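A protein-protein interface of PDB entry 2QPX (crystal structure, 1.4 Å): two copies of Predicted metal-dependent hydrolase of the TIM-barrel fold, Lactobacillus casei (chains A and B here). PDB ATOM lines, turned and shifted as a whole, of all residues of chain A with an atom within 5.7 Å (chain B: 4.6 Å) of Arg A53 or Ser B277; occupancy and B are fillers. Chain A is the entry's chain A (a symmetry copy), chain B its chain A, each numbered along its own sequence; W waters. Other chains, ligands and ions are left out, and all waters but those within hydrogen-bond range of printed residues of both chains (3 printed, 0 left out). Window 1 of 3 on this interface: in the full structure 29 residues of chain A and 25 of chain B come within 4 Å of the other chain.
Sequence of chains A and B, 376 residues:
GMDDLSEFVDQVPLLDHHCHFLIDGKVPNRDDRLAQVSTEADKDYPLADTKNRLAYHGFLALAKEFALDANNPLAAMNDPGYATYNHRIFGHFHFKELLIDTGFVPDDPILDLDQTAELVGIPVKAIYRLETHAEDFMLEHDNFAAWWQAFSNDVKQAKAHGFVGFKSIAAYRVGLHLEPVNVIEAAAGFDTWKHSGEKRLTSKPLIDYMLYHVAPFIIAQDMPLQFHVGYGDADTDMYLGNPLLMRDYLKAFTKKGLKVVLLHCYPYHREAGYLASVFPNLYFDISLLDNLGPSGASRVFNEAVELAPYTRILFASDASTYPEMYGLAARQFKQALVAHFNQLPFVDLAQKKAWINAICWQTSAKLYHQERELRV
The guanidinium group of Arg A53 lies within hydrogen-bond range of the backbone carbonyl oxygen of Leu A292 (3.0 Å). OG1 of Thr A39 sits at hydrogen-bond distance from N of Ala A41 (3.1 Å). OG of Ser B277 sits at hydrogen-bond distance from O of Tyr B274. The guanidinium group of Arg A53 sits at hydrogen-bond distance from the backbone carbonyl oxygen of Ser A38, 2.8 Å away. OH of Tyr A231 is in hydrogen-bond range of NH2 of Arg A53.
Among the printed residues, merely in contact across the chains: Thr A39 with Ser B277, Ala A41 with Ser B277, Ala A41 with Val B278, Tyr A45 with Ser B277, Tyr A45 with Val B278, Tyr A45 with Phe B279, Tyr A45 with Pro B309, Asp A49 with Pro B309, Asn A52 with Pro B309, Arg A53 with Ser B277, Arg A53 with Pro B309, Tyr A231 with Tyr B274, Tyr A231 with Leu B307, Leu A292 with Leu B307 and Gly A293 with Leu B307.
O of Ala B276 is in hydrogen-bond range of OH of Tyr A45, 2.7 Å away. The backbone carbonyl oxygen (O) of Leu B307 sits at hydrogen-bond distance from the guanidinium group (NE) of Arg A53 (2.8 Å).
Of the 17 printed residues of chain A, 9 touch a printed residue of chain B. Hydrophobic or aromatic side chains of chain A within 4 Å of the printed part of chain B: Ala A41, Tyr A45 and Tyr A231. Printed residues of chain B that touch a printed residue of chain A: Tyr B274, Ala B276, Ser B277, Val B278, Phe B279, Leu B307 and Pro B309. Among the printed residues, 17 pairs touch across the chains.
Water W1 lies within hydrogen-bond range of OG1 of Thr A39 (2.6 Å), O of Ser B277 (2.8 Å) and OG1 of Thr A50 (2.9 Å). Water W3 lies within hydrogen-bond range of the side-chain hydroxyl of Tyr A231 (2.7 Å), the side-chain hydroxyl of Thr A39 (2.9 Å), the side-chain hydroxyl of Ser B277 (3.0 Å) and the backbone NH of Glu A40 (3.3 Å). Water W2 lies within hydrogen-bond range of O of Ala B308 (2.9 Å) and N of Leu A54 (3.1 Å).
No position is printed for both chains.
Arg A53 touches just these residues of chain B: Ser B277, Leu B307 and Pro B309. Of the printed residues of chain B, Tyr A231 touches Tyr B274 and Leu B307. Of the printed residues of chain B, Asn A52 touches Pro B309. Thr A50 touches none of the printed residues of chain B. The nearest residue of chain B that does not touch Arg A53 is Ala B308 (4.04 Å). The nearest residue of chain A that does not touch Ser B277 is Tyr A231 (4.8 Å). The nearest printed residue of chain A that does not touch Tyr B274 is Glu A40 (5.8 Å).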
ATOM      1  N   SER A  38      -1.017  18.165 -23.377  1.00  0.00           N
ATOM      2  CA  SER A  38      -1.839  19.338 -23.632  1.00  0.00           C
ATOM      3  C   SER A  38      -2.627  19.815 -22.423  1.00  0.00           C
ATOM      4  O   SER A  38      -3.350  20.816 -22.518  1.00  0.00           O
ATOM      5  CB  SER A  38      -2.812  19.074 -24.786  1.00  0.00           C
ATOM      6  OG  SER A  38      -3.869  18.217 -24.395  1.00  0.00           O
ATOM      7  N   THR A  39      -2.468  19.127 -21.288  1.00  0.00           N
ATOM      8  CA  THR A  39      -3.213  19.420 -20.071  1.00  0.00           C
ATOM      9  C   THR A  39      -2.357  19.096 -18.867  1.00  0.00           C
ATOM     10  O   THR A  39      -1.408  18.331 -18.976  1.00  0.00           O
ATOM     11  CB  THR A  39      -4.511  18.548 -19.989  1.00  0.00           C
ATOM     12  OG1 THR A  39      -5.266  18.881 -18.819  1.00  0.00           O
ATOM     13  CG2 THR A  39      -4.194  17.038 -19.986  1.00  0.00           C
ATOM     14  N   GLU A  40      -2.696  19.671 -17.723  1.00  0.00           N
ATOM     15  CA  GLU A  40      -2.084  19.300 -16.456  1.00  0.00           C
ATOM     16  C   GLU A  40      -2.795  18.172 -15.716  1.00  0.00           C
ATOM     17  O   GLU A  40      -2.362  17.773 -14.634  1.00  0.00           O
ATOM     18  CB  GLU A  40      -1.948  20.546 -15.565  1.00  0.00           C
ATOM     19  CG  GLU A  40      -1.015  21.571 -16.211  1.00  0.00           C
ATOM     20  CD  GLU A  40       0.362  20.963 -16.553  1.00  0.00           C
ATOM     21  OE1 GLU A  40       0.998  20.435 -15.630  1.00  0.00           O
ATOM     22  OE2 GLU A  40       0.809  20.999 -17.725  1.00  0.00           O
ATOM     23  N   ALA A  41      -3.857  17.626 -16.303  1.00  0.00           N
ATOM     24  CA  ALA A  41      -4.533  16.472 -15.738  1.00  0.00           C
ATOM     25  C   ALA A  41      -3.564  15.285 -15.690  1.00  0.00           C
ATOM     26  O   ALA A  41      -2.628  15.201 -16.503  1.00  0.00           O
ATOM     27  CB  ALA A  41      -5.790  16.104 -16.573  1.00  0.00           C
ATOM     28  N   TYR A  45      -7.070  10.737 -15.531  1.00  0.00           N
ATOM     29  CA  TYR A  45      -8.137  11.607 -16.053  1.00  0.00           C
ATOM     30  C   TYR A  45      -8.520  11.126 -17.458  1.00  0.00           C
ATOM     31  O   TYR A  45      -7.636  10.769 -18.237  1.00  0.00           O
ATOM     32  CB  TYR A  45      -7.618  13.043 -16.096  1.00  0.00           C
ATOM     33  CG  TYR A  45      -8.588  14.098 -16.570  1.00  0.00           C
ATOM     34  CD1 TYR A  45      -8.740  14.385 -17.918  1.00  0.00           C
ATOM     35  CD2 TYR A  45      -9.308  14.874 -15.663  1.00  0.00           C
ATOM     36  CE1 TYR A  45      -9.583  15.391 -18.365  1.00  0.00           C
ATOM     37  CE2 TYR A  45     -10.143  15.879 -16.076  1.00  0.00           C
ATOM     38  CZ  TYR A  45     -10.313  16.136 -17.447  1.00  0.00           C
ATOM     39  OH  TYR A  45     -11.108  17.159 -17.922  1.00  0.00           O
ATOM     40  N   ASP A  49     -11.860  13.329 -22.478  1.00  0.00           N
ATOM     41  CA  ASP A  49     -12.179  14.676 -21.979  1.00  0.00           C
ATOM     42  C   ASP A  49     -11.064  15.678 -22.311  1.00  0.00           C
ATOM     43  O   ASP A  49     -11.320  16.793 -22.728  1.00  0.00           O
ATOM     44  CB  ASP A  49     -12.429  14.631 -20.470  1.00  0.00           C
ATOM     45  CG  ASP A  49     -13.640  13.778 -20.065  1.00  0.00           C
ATOM     46  OD1 ASP A  49     -14.426  13.323 -20.897  1.00  0.00           O
ATOM     47  OD2 ASP A  49     -13.800  13.553 -18.855  1.00  0.00           O
ATOM     48  N   THR A  50      -9.798  15.273 -22.115  1.00  0.00           N
ATOM     49  CA  THR A  50      -8.684  16.100 -22.503  1.00  0.00           C
ATOM     50  C   THR A  50      -8.766  16.474 -23.982  1.00  0.00           C
ATOM     51  O   THR A  50      -8.468  17.600 -24.360  1.00  0.00           O
ATOM     52  CB  THR A  50      -7.363  15.385 -22.173  1.00  0.00           C
ATOM     53  OG1 THR A  50      -7.272  15.277 -20.743  1.00  0.00           O
ATOM     54  CG2 THR A  50      -6.126  16.136 -22.775  1.00  0.00           C
ATOM     55  N   LYS A  51      -9.162  15.521 -24.817  1.00  0.00           N
ATOM     56  CA  LYS A  51      -9.248  15.743 -26.273  1.00  0.00           C
ATOM     57  C   LYS A  51     -10.421  16.640 -26.675  1.00  0.00           C
ATOM     58  O   LYS A  51     -10.524  17.052 -27.823  1.00  0.00           O
ATOM     59  CB  LYS A  51      -9.285  14.405 -27.023  1.00  0.00           C
ATOM     60  CG  LYS A  51      -7.963  13.675 -26.997  1.00  0.00           C
ATOM     61  CD  LYS A  51      -8.017  12.349 -27.763  1.00  0.00           C
ATOM     62  CE  LYS A  51      -6.667  11.677 -27.803  1.00  0.00           C
ATOM     63  NZ  LYS A  51      -6.756  10.287 -28.338  1.00  0.00           N
ATOM     64  N   ASN A  52     -11.288  16.960 -25.708  1.00  0.00           N
ATOM     65  CA  ASN A  52     -12.366  17.890 -25.911  1.00  0.00           C
ATOM     66  C   ASN A  52     -12.088  19.288 -25.361  1.00  0.00           C
ATOM     67  O   ASN A  52     -13.002  20.117 -25.216  1.00  0.00           O
ATOM     68  CB  ASN A  52     -13.700  17.297 -25.383  1.00  0.00           C
ATOM     69  CG  ASN A  52     -14.326  16.323 -26.363  1.00  0.00           C
ATOM     70  OD1 ASN A  52     -14.508  15.148 -26.055  1.00  0.00           O
ATOM     71  ND2 ASN A  52     -14.640  16.803 -27.537  1.00  0.00           N
ATOM     72  N   ARG A  53     -10.830  19.580 -25.096  1.00  0.00           N
ATOM     73  CA  ARG A  53     -10.325  20.918 -24.825  1.00  0.00           C
ATOM     74  C   ARG A  53      -9.720  21.471 -26.077  1.00  0.00           C
ATOM     75  O   ARG A  53      -9.229  20.706 -26.924  1.00  0.00           O
ATOM     76  CB  ARG A  53      -9.250  20.874 -23.740  1.00  0.00           C
ATOM     77  CG  ARG A  53      -9.738  20.252 -22.431  1.00  0.00           C
ATOM     78  CD  ARG A  53      -8.633  20.088 -21.415  1.00  0.00           C
ATOM     79  NE  ARG A  53      -8.077  21.348 -20.962  1.00  0.00           N
ATOM     80  CZ  ARG A  53      -6.878  21.839 -21.262  1.00  0.00           C
ATOM     81  NH1 ARG A  53      -6.052  21.247 -22.104  1.00  0.00           N
ATOM     82  NH2 ARG A  53      -6.490  22.946 -20.688  1.00  0.00           N
ATOM     83  N   LEU A  54      -9.648  22.793 -26.164  1.00  0.00           N
ATOM     84  CA  LEU A  54      -9.117  23.437 -27.343  1.00  0.00           C
ATOM     85  C   LEU A  54      -7.611  23.206 -27.546  1.00  0.00           C
ATOM     86  O   LEU A  54      -7.159  23.095 -28.709  1.00  0.00           O
ATOM     87  CB  LEU A  54      -9.422  24.936 -27.322  1.00  0.00           C
ATOM     88  CG  LEU A  54      -9.264  25.667 -28.658  1.00  0.00           C
ATOM     89  CD1 LEU A  54     -10.186  25.036 -29.749  1.00  0.00           C
ATOM     90  CD2 LEU A  54      -9.595  27.164 -28.532  1.00  0.00           C
ATOM     91  N   ALA A  55      -6.829  23.083 -26.477  1.00  0.00           N
ATOM     92  CA  ALA A  55      -5.375  22.965 -26.609  1.00  0.00           C
ATOM     93  C   ALA A  55      -4.974  21.794 -27.512  1.00  0.00           C
ATOM     94  O   ALA A  55      -4.100  21.915 -28.351  1.00  0.00           O
ATOM     95  CB  ALA A  55      -4.696  22.825 -25.217  1.00  0.00           C
ATOM     96  N   TYR A  56      -5.595  20.642 -27.282  1.00  0.00           N
ATOM     97  CA  TYR A  56      -5.283  19.460 -28.087  1.00  0.00           C
ATOM     98  C   TYR A  56      -5.522  19.749 -29.560  1.00  0.00           C
ATOM     99  O   TYR A  56      -4.696  19.367 -30.427  1.00  0.00           O
ATOM    100  CB  TYR A  56      -6.089  18.262 -27.615  1.00  0.00           C
ATOM    101  CG  TYR A  56      -6.038  17.049 -28.528  1.00  0.00           C
ATOM    102  CD1 TYR A  56      -4.884  16.312 -28.689  1.00  0.00           C
ATOM    103  CD2 TYR A  56      -7.162  16.664 -29.224  1.00  0.00           C
ATOM    104  CE1 TYR A  56      -4.873  15.190 -29.531  1.00  0.00           C
ATOM    105  CE2 TYR A  56      -7.164  15.582 -30.044  1.00  0.00           C
ATOM    106  CZ  TYR A  56      -6.031  14.823 -30.185  1.00  0.00           C
ATOM    107  OH  TYR A  56      -6.051  13.710 -31.041  1.00  0.00           O
ATOM    108  N   HIS A  57      -6.647  20.378 -29.853  1.00  0.00           N
ATOM    109  CA  HIS A  57      -6.927  20.733 -31.252  1.00  0.00           C
ATOM    110  C   HIS A  57      -5.945  21.710 -31.848  1.00  0.00           C
ATOM    111  O   HIS A  57      -5.602  21.592 -33.045  1.00  0.00           O
ATOM    112  CB  HIS A  57      -8.365  21.183 -31.393  1.00  0.00           C
ATOM    113  CG  HIS A  57      -9.322  20.076 -31.130  1.00  0.00           C
ATOM    114  ND1 HIS A  57      -9.813  19.254 -32.122  1.00  0.00           N
ATOM    115  CD2 HIS A  57      -9.818  19.581 -29.958  1.00  0.00           C
ATOM    116  CE1 HIS A  57     -10.587  18.328 -31.579  1.00  0.00           C
ATOM    117  NE2 HIS A  57     -10.609  18.505 -30.264  1.00  0.00           N
ATOM    118  N   TYR A 231      -1.819  28.109 -12.137  1.00  0.00           N
ATOM    119  CA  TYR A 231      -2.117  26.890 -12.937  1.00  0.00           C
ATOM    120  C   TYR A 231      -1.198  25.703 -12.667  1.00  0.00           C
ATOM    121  O   TYR A 231      -0.094  25.663 -13.128  1.00  0.00           O
ATOM    122  CB  TYR A 231      -2.174  27.283 -14.428  1.00  0.00           C
ATOM    123  CG  TYR A 231      -2.717  26.274 -15.452  1.00  0.00           C
ATOM    124  CD1 TYR A 231      -3.306  25.070 -15.084  1.00  0.00           C
ATOM    125  CD2 TYR A 231      -2.569  26.538 -16.789  1.00  0.00           C
ATOM    126  CE1 TYR A 231      -3.779  24.179 -16.033  1.00  0.00           C
ATOM    127  CE2 TYR A 231      -3.011  25.647 -17.757  1.00  0.00           C
ATOM    128  CZ  TYR A 231      -3.610  24.469 -17.379  1.00  0.00           C
ATOM    129  OH  TYR A 231      -4.090  23.558 -18.322  1.00  0.00           O
ATOM    130  N   LEU A 292      -1.841  26.102 -23.298  1.00  0.00           N
ATOM    131  CA  LEU A 292      -2.856  25.109 -22.844  1.00  0.00           C
ATOM    132  C   LEU A 292      -4.228  25.711 -22.647  1.00  0.00           C
ATOM    133  O   LEU A 292      -5.232  24.988 -22.483  1.00  0.00           O
ATOM    134  CB  LEU A 292      -2.386  24.342 -21.595  1.00  0.00           C
ATOM    135  CG  LEU A 292      -1.021  23.620 -21.695  1.00  0.00           C
ATOM    136  CD1 LEU A 292      -0.903  22.571 -20.585  1.00  0.00           C
ATOM    137  CD2 LEU A 292      -0.825  22.989 -23.064  1.00  0.00           C
ATOM    138  N   GLY A 293      -4.295  27.032 -22.707  1.00  0.00           N
ATOM    139  CA  GLY A 293      -5.587  27.775 -22.678  1.00  0.00           C
ATOM    140  C   GLY A 293      -5.599  28.746 -23.831  1.00  0.00           C
ATOM    141  O   GLY A 293      -5.761  29.995 -23.654  1.00  0.00           O
ATOM    142  N   GLY B 273     -13.832  26.035 -14.261  1.00  0.00           N
ATOM    143  CA  GLY B 273     -13.370  25.457 -15.515  1.00  0.00           C
ATOM    144  C   GLY B 273     -12.017  24.791 -15.384  1.00  0.00           C
ATOM    145  O   GLY B 273     -11.778  23.726 -15.969  1.00  0.00           O
ATOM    146  N   TYR B 274     -11.123  25.415 -14.628  1.00  0.00           N
ATOM    147  CA  TYR B 274      -9.856  24.785 -14.250  1.00  0.00           C
ATOM    148  C   TYR B 274     -10.105  23.437 -13.570  1.00  0.00           C
ATOM    149  O   TYR B 274      -9.515  22.412 -13.964  1.00  0.00           O
ATOM    150  CB  TYR B 274      -9.000  25.724 -13.375  1.00  0.00           C
ATOM    151  CG  TYR B 274      -7.921  24.948 -12.664  1.00  0.00           C
ATOM    152  CD1 TYR B 274      -6.829  24.472 -13.349  1.00  0.00           C
ATOM    153  CD2 TYR B 274      -8.091  24.576 -11.331  1.00  0.00           C
ATOM    154  CE1 TYR B 274      -5.903  23.648 -12.705  1.00  0.00           C
ATOM    155  CE2 TYR B 274      -7.171  23.788 -10.681  1.00  0.00           C
ATOM    156  CZ  TYR B 274      -6.086  23.333 -11.362  1.00  0.00           C
ATOM    157  OH  TYR B 274      -5.174  22.522 -10.719  1.00  0.00           O
ATOM    158  N   LEU B 275     -10.970  23.417 -12.555  1.00  0.00           N
ATOM    159  CA  LEU B 275     -11.262  22.173 -11.861  1.00  0.00           C
ATOM    160  C   LEU B 275     -11.807  21.084 -12.808  1.00  0.00           C
ATOM    161  O   LEU B 275     -11.413  19.930 -12.719  1.00  0.00           O
ATOM    162  CB  LEU B 275     -12.202  22.376 -10.685  1.00  0.00           C
ATOM    163  CG  LEU B 275     -11.642  23.188  -9.536  1.00  0.00           C
ATOM    164  CD1 LEU B 275     -12.822  23.584  -8.632  1.00  0.00           C
ATOM    165  CD2 LEU B 275     -10.581  22.369  -8.774  1.00  0.00           C
ATOM    166  N   ALA B 276     -12.621  21.485 -13.781  1.00  0.00           N
ATOM    167  CA  ALA B 276     -13.172  20.564 -14.754  1.00  0.00           C
ATOM    168  C   ALA B 276     -12.060  19.942 -15.606  1.00  0.00           C
ATOM    169  O   ALA B 276     -12.184  18.828 -16.047  1.00  0.00           O
ATOM    170  CB  ALA B 276     -14.220  21.252 -15.623  1.00  0.00           C
ATOM    171  N   SER B 277     -10.989  20.683 -15.831  1.00  0.00           N
ATOM    172  CA  SER B 277      -9.858  20.238 -16.629  1.00  0.00           C
ATOM    173  C   SER B 277      -8.942  19.245 -15.933  1.00  0.00           C
ATOM    174  O   SER B 277      -8.155  18.589 -16.611  1.00  0.00           O
ATOM    175  CB  SER B 277      -9.039  21.438 -17.142  1.00  0.00           C
ATOM    176  OG  SER B 277      -8.096  21.956 -16.193  1.00  0.00           O
ATOM    177  N   VAL B 278      -9.032  19.134 -14.603  1.00  0.00           N
ATOM    178  CA  VAL B 278      -8.117  18.250 -13.843  1.00  0.00           C
ATOM    179  C   VAL B 278      -8.813  17.204 -12.973  1.00  0.00           C
ATOM    180  O   VAL B 278      -8.147  16.310 -12.485  1.00  0.00           O
ATOM    181  CB  VAL B 278      -7.059  19.052 -13.048  1.00  0.00           C
ATOM    182  CG1 VAL B 278      -6.129  19.880 -13.971  1.00  0.00           C
ATOM    183  CG2 VAL B 278      -7.728  19.966 -11.995  1.00  0.00           C
ATOM    184  N   PHE B 279     -10.126  17.291 -12.762  1.00  0.00           N
ATOM    185  CA  PHE B 279     -10.869  16.255 -12.057  1.00  0.00           C
ATOM    186  C   PHE B 279     -11.806  15.499 -12.976  1.00  0.00           C
ATOM    187  O   PHE B 279     -12.481  16.117 -13.782  1.00  0.00           O
ATOM    188  CB  PHE B 279     -11.704  16.849 -10.879  1.00  0.00           C
ATOM    189  CG  PHE B 279     -10.864  17.228  -9.692  1.00  0.00           C
ATOM    190  CD1 PHE B 279     -10.511  16.267  -8.757  1.00  0.00           C
ATOM    191  CD2 PHE B 279     -10.382  18.509  -9.541  1.00  0.00           C
ATOM    192  CE1 PHE B 279      -9.679  16.591  -7.684  1.00  0.00           C
ATOM    193  CE2 PHE B 279      -9.585  18.847  -8.461  1.00  0.00           C
ATOM    194  CZ  PHE B 279      -9.234  17.886  -7.540  1.00  0.00           C
ATOM    195  N   LEU B 307      -9.835  26.913 -20.050  1.00  0.00           N
ATOM    196  CA  LEU B 307      -9.186  25.639 -19.774  1.00  0.00           C
ATOM    197  C   LEU B 307     -10.115  24.449 -19.752  1.00  0.00           C
ATOM    198  O   LEU B 307      -9.668  23.345 -19.845  1.00  0.00           O
ATOM    199  CB  LEU B 307      -8.473  25.660 -18.412  1.00  0.00           C
ATOM    200  CG  LEU B 307      -7.319  26.639 -18.222  1.00  0.00           C
ATOM    201  CD1 LEU B 307      -6.748  26.521 -16.803  1.00  0.00           C
ATOM    202  CD2 LEU B 307      -6.244  26.450 -19.274  1.00  0.00           C
ATOM    203  N   ALA B 308     -11.413  24.643 -19.584  1.00  0.00           N
ATOM    204  CA  ALA B 308     -12.308  23.505 -19.436  1.00  0.00           C
ATOM    205  C   ALA B 308     -12.445  22.719 -20.724  1.00  0.00           C
ATOM    206  O   ALA B 308     -12.459  23.296 -21.818  1.00  0.00           O
ATOM    207  CB  ALA B 308     -13.740  24.010 -19.056  1.00  0.00           C
ATOM    208  N   PRO B 309     -12.754  21.427 -20.604  1.00  0.00           N
ATOM    209  CA  PRO B 309     -13.268  20.727 -21.780  1.00  0.00           C
ATOM    210  C   PRO B 309     -14.679  21.232 -22.100  1.00  0.00           C
ATOM    211  O   PRO B 309     -15.481  21.443 -21.200  1.00  0.00           O
ATOM    212  CB  PRO B 309     -13.339  19.273 -21.322  1.00  0.00           C
ATOM    213  CG  PRO B 309     -12.496  19.202 -20.080  1.00  0.00           C
ATOM    214  CD  PRO B 309     -12.692  20.528 -19.449  1.00  0.00           C
HETATM  215  O   HOH W   1      -7.613  17.768 -19.254  1.00  0.00           O
HETATM  216  O   HOH W   2     -10.626  24.378 -23.740  1.00  0.00           O
HETATM  217  O   HOH W   3      -5.439  21.397 -17.413  1.00  0.00           O
